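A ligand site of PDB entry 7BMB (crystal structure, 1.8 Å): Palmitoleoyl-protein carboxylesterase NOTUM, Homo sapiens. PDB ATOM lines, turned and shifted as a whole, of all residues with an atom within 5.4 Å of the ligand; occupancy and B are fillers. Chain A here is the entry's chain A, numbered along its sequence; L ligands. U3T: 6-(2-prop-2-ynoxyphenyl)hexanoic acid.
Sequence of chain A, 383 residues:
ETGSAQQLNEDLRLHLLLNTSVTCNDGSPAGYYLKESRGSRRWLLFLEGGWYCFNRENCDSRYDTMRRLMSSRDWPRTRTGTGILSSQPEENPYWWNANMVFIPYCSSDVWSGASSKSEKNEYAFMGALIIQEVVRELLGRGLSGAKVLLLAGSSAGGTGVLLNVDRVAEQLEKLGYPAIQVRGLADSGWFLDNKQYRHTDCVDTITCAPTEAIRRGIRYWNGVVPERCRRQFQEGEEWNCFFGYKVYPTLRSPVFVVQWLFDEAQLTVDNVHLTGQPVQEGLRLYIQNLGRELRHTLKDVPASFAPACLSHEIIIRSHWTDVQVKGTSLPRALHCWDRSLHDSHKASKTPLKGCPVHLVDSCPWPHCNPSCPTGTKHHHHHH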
ATOM      1  N   GLY A  49       8.309  24.654  17.798  1.00  0.00           N
ATOM      2  CA  GLY A  49       7.512  25.817  18.128  1.00  0.00           C
ATOM      3  C   GLY A  49       8.337  26.932  18.769  1.00  0.00           C
ATOM      4  O   GLY A  49       9.576  26.893  18.819  1.00  0.00           O
ATOM      5  N   GLY A  50       7.632  27.941  19.275  1.00  0.00           N
ATOM      6  CA  GLY A  50       8.263  29.037  19.989  1.00  0.00           C
ATOM      7  C   GLY A  50       7.650  30.407  19.763  1.00  0.00           C
ATOM      8  O   GLY A  50       8.383  31.380  19.579  1.00  0.00           O
ATOM      9  N   TRP A  51       6.325  30.502  19.786  1.00  0.00           N
ATOM     10  CA  TRP A  51       5.596  31.779  19.613  1.00  0.00           C
ATOM     11  C   TRP A  51       5.961  32.381  18.247  1.00  0.00           C
ATOM     12  O   TRP A  51       6.065  31.651  17.246  1.00  0.00           O
ATOM     13  CB  TRP A  51       5.876  32.704  20.797  1.00  0.00           C
ATOM     14  CG  TRP A  51       5.246  32.244  22.088  1.00  0.00           C
ATOM     15  CD1 TRP A  51       5.852  31.596  23.111  1.00  0.00           C
ATOM     16  CD2 TRP A  51       3.871  32.387  22.468  1.00  0.00           C
ATOM     17  NE1 TRP A  51       4.956  31.338  24.113  1.00  0.00           N
ATOM     18  CE2 TRP A  51       3.724  31.806  23.743  1.00  0.00           C
ATOM     19  CE3 TRP A  51       2.737  32.950  21.853  1.00  0.00           C
ATOM     20  CZ2 TRP A  51       2.504  31.769  24.415  1.00  0.00           C
ATOM     21  CZ3 TRP A  51       1.532  32.919  22.529  1.00  0.00           C
ATOM     22  CH2 TRP A  51       1.421  32.331  23.801  1.00  0.00           C
ATOM     23  N   TYR A  52       6.115  33.706  18.158  1.00  0.00           N
ATOM     24  CA  TYR A  52       6.363  34.407  16.913  1.00  0.00           C
ATOM     25  C   TYR A  52       6.613  35.871  17.201  1.00  0.00           C
ATOM     26  O   TYR A  52       6.540  36.290  18.366  1.00  0.00           O
ATOM     27  CB  TYR A  52       5.185  34.265  15.938  1.00  0.00           C
ATOM     28  CG  TYR A  52       3.857  34.713  16.493  1.00  0.00           C
ATOM     29  CD1 TYR A  52       3.044  33.841  17.198  1.00  0.00           C
ATOM     30  CD2 TYR A  52       3.386  36.008  16.267  1.00  0.00           C
ATOM     31  CE1 TYR A  52       1.810  34.237  17.692  1.00  0.00           C
ATOM     32  CE2 TYR A  52       2.155  36.414  16.764  1.00  0.00           C
ATOM     33  CZ  TYR A  52       1.373  35.522  17.475  1.00  0.00           C
ATOM     34  OH  TYR A  52       0.149  35.928  17.966  1.00  0.00           O
ATOM     35  N   VAL A 110       5.029  31.336  12.622  1.00  0.00           N
ATOM     36  CA  VAL A 110       4.133  30.185  12.737  1.00  0.00           C
ATOM     37  C   VAL A 110       4.185  29.373  11.439  1.00  0.00           C
ATOM     38  O   VAL A 110       3.183  28.795  11.013  1.00  0.00           O
ATOM     39  CB  VAL A 110       2.683  30.623  13.077  1.00  0.00           C
ATOM     40  CG1 VAL A 110       1.878  29.450  13.649  1.00  0.00           C
ATOM     41  CG2 VAL A 110       2.695  31.804  14.059  1.00  0.00           C
ATOM     42  N   SER A 154       4.897  20.996  17.387  1.00  0.00           N
ATOM     43  CA  SER A 154       4.397  21.349  18.711  1.00  0.00           C
ATOM     44  C   SER A 154       4.272  22.861  18.834  1.00  0.00           C
ATOM     45  O   SER A 154       5.140  23.599  18.358  1.00  0.00           O
ATOM     46  CB  SER A 154       5.307  20.800  19.815  1.00  0.00           C
ATOM     47  OG  SER A 154       5.256  19.384  19.883  1.00  0.00           O
ATOM     48  N   SER A 155       3.206  23.311  19.490  1.00  0.00           N
ATOM     49  CA  SER A 155       2.940  24.732  19.785  1.00  0.00           C
ATOM     50  C   SER A 155       2.800  25.463  18.457  1.00  0.00           C
ATOM     51  O   SER A 155       1.960  25.064  17.643  1.00  0.00           O
ATOM     52  CB  SER A 155       4.002  25.274  20.726  1.00  0.00           C
ATOM     53  OG  SER A 155       3.998  24.573  21.947  1.00  0.00           O
ATOM     54  N   ALA A 156       3.578  26.537  18.211  1.00  0.00           N
ATOM     55  CA  ALA A 156       3.562  27.150  16.887  1.00  0.00           C
ATOM     56  C   ALA A 156       3.890  26.145  15.792  1.00  0.00           C
ATOM     57  O   ALA A 156       3.433  26.302  14.656  1.00  0.00           O
ATOM     58  CB  ALA A 156       4.573  28.310  16.826  1.00  0.00           C
ATOM     59  N   GLY A 157       4.692  25.117  16.102  1.00  0.00           N
ATOM     60  CA  GLY A 157       4.938  24.062  15.127  1.00  0.00           C
ATOM     61  C   GLY A 157       3.705  23.229  14.836  1.00  0.00           C
ATOM     62  O   GLY A 157       3.537  22.739  13.709  1.00  0.00           O
ATOM     63  N   THR A 159       0.508  24.420  14.980  1.00  0.00           N
ATOM     64  CA  THR A 159      -0.261  25.236  14.040  1.00  0.00           C
ATOM     65  C   THR A 159       0.367  25.157  12.644  1.00  0.00           C
ATOM     66  O   THR A 159      -0.348  25.094  11.629  1.00  0.00           O
ATOM     67  CB  THR A 159      -0.344  26.677  14.549  1.00  0.00           C
ATOM     68  OG1 THR A 159      -0.820  26.673  15.904  1.00  0.00           O
ATOM     69  CG2 THR A 159      -1.311  27.493  13.694  1.00  0.00           C
ATOM     70  N   SER A 188      -0.490  20.685  20.503  1.00  0.00           N
ATOM     71  CA  SER A 188      -0.592  21.978  21.208  1.00  0.00           C
ATOM     72  C   SER A 188      -0.628  23.167  20.248  1.00  0.00           C
ATOM     73  O   SER A 188      -0.129  24.255  20.548  1.00  0.00           O
ATOM     74  CB  SER A 188       0.536  22.139  22.218  1.00  0.00           C
ATOM     75  OG  SER A 188       0.514  21.099  23.166  1.00  0.00           O
ATOM     76  N   GLY A 189      -1.276  22.973  19.107  1.00  0.00           N
ATOM     77  CA  GLY A 189      -1.405  24.056  18.162  1.00  0.00           C
ATOM     78  C   GLY A 189      -2.842  24.392  17.824  1.00  0.00           C
ATOM     79  O   GLY A 189      -3.099  25.066  16.820  1.00  0.00           O
ATOM     80  N   PHE A 191      -5.971  26.285  18.945  1.00  0.00           N
ATOM     81  CA  PHE A 191      -6.343  27.384  19.822  1.00  0.00           C
ATOM     82  C   PHE A 191      -7.721  27.930  19.499  1.00  0.00           C
ATOM     83  O   PHE A 191      -8.266  27.726  18.411  1.00  0.00           O
ATOM     84  CB  PHE A 191      -5.315  28.517  19.732  1.00  0.00           C
ATOM     85  CG  PHE A 191      -3.945  28.074  20.105  1.00  0.00           C
ATOM     86  CD1 PHE A 191      -2.980  27.865  19.135  1.00  0.00           C
ATOM     87  CD2 PHE A 191      -3.642  27.781  21.424  1.00  0.00           C
ATOM     88  CE1 PHE A 191      -1.729  27.435  19.483  1.00  0.00           C
ATOM     89  CE2 PHE A 191      -2.388  27.338  21.776  1.00  0.00           C
ATOM     90  CZ  PHE A 191      -1.437  27.155  20.805  1.00  0.00           C
ATOM     91  N   LEU A 192      -8.265  28.645  20.477  1.00  0.00           N
ATOM     92  CA  LEU A 192      -9.574  29.279  20.371  1.00  0.00           C
ATOM     93  C   LEU A 192      -9.380  30.782  20.336  1.00  0.00           C
ATOM     94  O   LEU A 192      -8.592  31.342  21.128  1.00  0.00           O
ATOM     95  CB  LEU A 192     -10.477  28.883  21.537  1.00  0.00           C
ATOM     96  CG  LEU A 192     -10.682  27.376  21.758  1.00  0.00           C
ATOM     97  CD1 LEU A 192     -11.507  27.116  23.008  1.00  0.00           C
ATOM     98  CD2 LEU A 192     -11.345  26.723  20.539  1.00  0.00           C
ATOM     99  N   PRO A 210      -4.559  37.290  20.305  1.00  0.00           N
ATOM    100  CA  PRO A 210      -4.052  36.508  19.152  1.00  0.00           C
ATOM    101  C   PRO A 210      -4.578  36.986  17.819  1.00  0.00           C
ATOM    102  O   PRO A 210      -3.802  37.100  16.859  1.00  0.00           O
ATOM    103  CB  PRO A 210      -4.545  35.084  19.465  1.00  0.00           C
ATOM    104  CG  PRO A 210      -4.730  35.057  20.941  1.00  0.00           C
ATOM    105  CD  PRO A 210      -5.171  36.435  21.333  1.00  0.00           C
ATOM    106  N   ILE A 214      -1.934  37.967  15.173  1.00  0.00           N
ATOM    107  CA  ILE A 214      -1.882  37.139  13.975  1.00  0.00           C
ATOM    108  C   ILE A 214      -2.258  37.951  12.740  1.00  0.00           C
ATOM    109  O   ILE A 214      -1.609  37.853  11.691  1.00  0.00           O
ATOM    110  CB  ILE A 214      -2.776  35.890  14.117  1.00  0.00           C
ATOM    111  CG1 ILE A 214      -2.175  34.922  15.119  1.00  0.00           C
ATOM    112  CG2 ILE A 214      -2.947  35.192  12.766  1.00  0.00           C
ATOM    113  CD1 ILE A 214      -3.188  33.995  15.685  1.00  0.00           C
ATOM    114  N   PHE A 242      -5.432  30.271  10.966  1.00  0.00           N
ATOM    115  CA  PHE A 242      -4.499  29.911  12.018  1.00  0.00           C
ATOM    116  C   PHE A 242      -5.169  29.228  13.202  1.00  0.00           C
ATOM    117  O   PHE A 242      -4.472  28.778  14.112  1.00  0.00           O
ATOM    118  CB  PHE A 242      -3.747  31.154  12.540  1.00  0.00           C
ATOM    119  CG  PHE A 242      -2.640  31.611  11.637  1.00  0.00           C
ATOM    120  CD1 PHE A 242      -2.919  32.076  10.367  1.00  0.00           C
ATOM    121  CD2 PHE A 242      -1.318  31.581  12.069  1.00  0.00           C
ATOM    122  CE1 PHE A 242      -1.897  32.482   9.530  1.00  0.00           C
ATOM    123  CE2 PHE A 242      -0.300  32.001  11.228  1.00  0.00           C
ATOM    124  CZ  PHE A 242      -0.594  32.460   9.953  1.00  0.00           C
ATOM    125  N   PHE A 243      -6.492  29.152  13.212  1.00  0.00           N
ATOM    126  CA  PHE A 243      -7.225  28.531  14.299  1.00  0.00           C
ATOM    127  C   PHE A 243      -7.718  27.156  13.862  1.00  0.00           C
ATOM    128  O   PHE A 243      -8.550  27.044  12.952  1.00  0.00           O
ATOM    129  CB  PHE A 243      -8.370  29.436  14.757  1.00  0.00           C
ATOM    130  CG  PHE A 243      -7.860  30.675  15.424  1.00  0.00           C
ATOM    131  CD1 PHE A 243      -7.463  31.771  14.684  1.00  0.00           C
ATOM    132  CD2 PHE A 243      -7.660  30.689  16.801  1.00  0.00           C
ATOM    133  CE1 PHE A 243      -6.925  32.900  15.310  1.00  0.00           C
ATOM    134  CE2 PHE A 243      -7.148  31.807  17.441  1.00  0.00           C
ATOM    135  CZ  PHE A 243      -6.776  32.915  16.686  1.00  0.00           C
ATOM    136  N   ALA A 265      -0.534  27.915  26.903  1.00  0.00           N
ATOM    137  CA  ALA A 265      -0.420  29.047  26.004  1.00  0.00           C
ATOM    138  C   ALA A 265      -1.781  29.695  25.779  1.00  0.00           C
ATOM    139  O   ALA A 265      -1.884  30.919  25.670  1.00  0.00           O
ATOM    140  CB  ALA A 265       0.206  28.615  24.675  1.00  0.00           C
ATOM    141  N   GLN A 266      -2.837  28.871  25.676  1.00  0.00           N
ATOM    142  CA  GLN A 266      -4.194  29.394  25.629  1.00  0.00           C
ATOM    143  C   GLN A 266      -4.523  30.221  26.875  1.00  0.00           C
ATOM    144  O   GLN A 266      -5.078  31.318  26.784  1.00  0.00           O
ATOM    145  CB  GLN A 266      -5.183  28.226  25.501  1.00  0.00           C
ATOM    146  CG  GLN A 266      -6.627  28.658  25.430  1.00  0.00           C
ATOM    147  CD  GLN A 266      -6.978  29.206  24.069  1.00  0.00           C
ATOM    148  OE1 GLN A 266      -6.785  28.537  23.059  1.00  0.00           O
ATOM    149  NE2 GLN A 266      -7.518  30.417  24.044  1.00  0.00           N
ATOM    150  N   VAL A 269      -2.594  33.758  26.825  1.00  0.00           N
ATOM    151  CA  VAL A 269      -3.202  34.784  25.987  1.00  0.00           C
ATOM    152  C   VAL A 269      -4.587  35.169  26.510  1.00  0.00           C
ATOM    153  O   VAL A 269      -5.042  36.286  26.255  1.00  0.00           O
ATOM    154  CB  VAL A 269      -3.247  34.336  24.510  1.00  0.00           C
ATOM    155  CG1 VAL A 269      -1.846  34.024  24.015  1.00  0.00           C
ATOM    156  CG2 VAL A 269      -4.175  33.150  24.311  1.00  0.00           C
ATOM    157  N   HIS A 312       1.591  22.076  28.460  1.00  0.00           N
ATOM    158  CA  HIS A 312       1.985  22.681  27.184  1.00  0.00           C
ATOM    159  C   HIS A 312       2.966  21.758  26.470  1.00  0.00           C
ATOM    160  O   HIS A 312       4.017  21.448  27.014  1.00  0.00           O
ATOM    161  CB  HIS A 312       2.629  24.052  27.404  1.00  0.00           C
ATOM    162  CG  HIS A 312       2.821  24.817  26.140  1.00  0.00           C
ATOM    163  ND1 HIS A 312       4.037  25.308  25.739  1.00  0.00           N
ATOM    164  CD2 HIS A 312       1.944  25.136  25.160  1.00  0.00           C
ATOM    165  CE1 HIS A 312       3.905  25.927  24.580  1.00  0.00           C
ATOM    166  NE2 HIS A 312       2.647  25.832  24.207  1.00  0.00           N
ATOM    167  N   GLU A 313       2.607  21.347  25.245  1.00  0.00           N
ATOM    168  CA  GLU A 313       3.363  20.415  24.397  1.00  0.00           C
ATOM    169  C   GLU A 313       3.378  19.007  24.973  1.00  0.00           C
ATOM    170  O   GLU A 313       3.119  18.816  26.151  1.00  0.00           O
ATOM    171  CB  GLU A 313       4.802  20.892  24.160  1.00  0.00           C
ATOM    172  CG  GLU A 313       4.884  22.267  23.559  1.00  0.00           C
ATOM    173  CD  GLU A 313       6.289  22.705  23.189  1.00  0.00           C
ATOM    174  OE1 GLU A 313       6.453  23.342  22.127  1.00  0.00           O
ATOM    175  OE2 GLU A 313       7.234  22.407  23.961  1.00  0.00           O
HETATM  176  C01 U3T L   1      -4.967  31.648  21.429  1.00  0.00           C
HETATM  177  C02 U3T L   1      -3.797  31.589  21.201  1.00  0.00           C
HETATM  178  C03 U3T L   1      -2.295  31.505  20.880  1.00  0.00           C
HETATM  179  C05 U3T L   1      -2.113  31.571  18.513  1.00  0.00           C
HETATM  180  C06 U3T L   1      -3.336  31.414  17.913  1.00  0.00           C
HETATM  181  C07 U3T L   1      -3.445  30.704  16.728  1.00  0.00           C
HETATM  182  C08 U3T L   1      -2.324  30.129  16.167  1.00  0.00           C
HETATM  183  C09 U3T L   1      -1.088  30.282  16.769  1.00  0.00           C
HETATM  184  C10 U3T L   1      -0.971  30.993  17.948  1.00  0.00           C
HETATM  185  C11 U3T L   1       0.398  31.134  18.592  1.00  0.00           C
HETATM  186  C12 U3T L   1       1.020  29.805  18.986  1.00  0.00           C
HETATM  187  C13 U3T L   1       2.102  29.977  20.052  1.00  0.00           C
HETATM  188  C14 U3T L   1       2.233  28.728  20.917  1.00  0.00           C
HETATM  189  C15 U3T L   1       3.337  28.811  21.972  1.00  0.00           C
HETATM  190  C16 U3T L   1       4.705  28.263  21.511  1.00  0.00           C
HETATM  191  O04 U3T L   1      -2.044  32.279  19.728  1.00  0.00           O
HETATM  192  O17 U3T L   1       4.967  28.221  20.283  1.00  0.00           O
HETATM  193  O18 U3T L   1       5.536  27.837  22.370  1.00  0.00           O
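The backbone NH (N) of Gly 50 sits at hydrogen-bond distance from an oxygen (O17) of the ligand (2.9 Å). The backbone NH of Ala 156 is in hydrogen-bond range of an oxygen (O17) of the ligand (3.0 Å). N of Trp 51 is in hydrogen-bond range of O17 of the ligand (2.7 Å).
The side-chain hydroxyl (OG) of Ser 155 lies within hydrogen-bond range of the side-chain carboxylate (OE1) of Glu 313 (2.8 Å). The backbone NH (N) of Gly 49 sits close to the backbone carbonyl oxygen (O) of Ser 154 (3.4 Å). OE1 of Gln 266 lies within hydrogen-bond range of N of Leu 192. The side-chain hydroxyl (OG) of Ser 155 is in hydrogen-bond range of a ring nitrogen (NE2) of His 312 (2.9 Å). O of Gly 189 is in hydrogen-bond range of OG1 of Thr 159.
C of Gly 49 touches O17 of the ligand, 3.9 Å away. CE1 of Tyr 52 touches C11 of the ligand, 3.5 Å away. CB of Ser 155 touches O17 of the ligand, at 3.1 Å. OG1 of Thr 159 touches C09 of the ligand (3.7 Å). Phe 191 touches the ligand (CB to C01, 3.6 Å). O of Leu 192 touches C01 of the ligand, 3.7 Å away. Pro 210 touches the ligand (CG to C01, 3.5 Å). CD1 of Ile 214 touches C06 of the ligand, 3.4 Å away. Phe 242 touches the ligand (O to C08, 3.3 Å). Phe 243 touches the ligand. Gln 266 touches the ligand (NE2 to C01, 3.9 Å). Val 269 touches the ligand. CE1 of His 312 touches O18 of the ligand, 3.3 Å away. Hydrophobic or aromatic side chains that line the ligand: Trp 51, Tyr 52, Ala 156, Phe 191, Pro 210, Ile 214, Phe 243, Val 269 and His 312. 16 residues have an atom within 4 Å of the ligand: Gly 49, Gly 50, Trp 51, Tyr 52, Ser 155, Ala 156, Thr 159, Phe 191, Leu 192, Pro 210, Ile 214, Phe 242, Phe 243, Gln 266, Val 269 and His 312. The nearest printed residue that does not touch the ligand is Ala 265 (4.1 Å).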
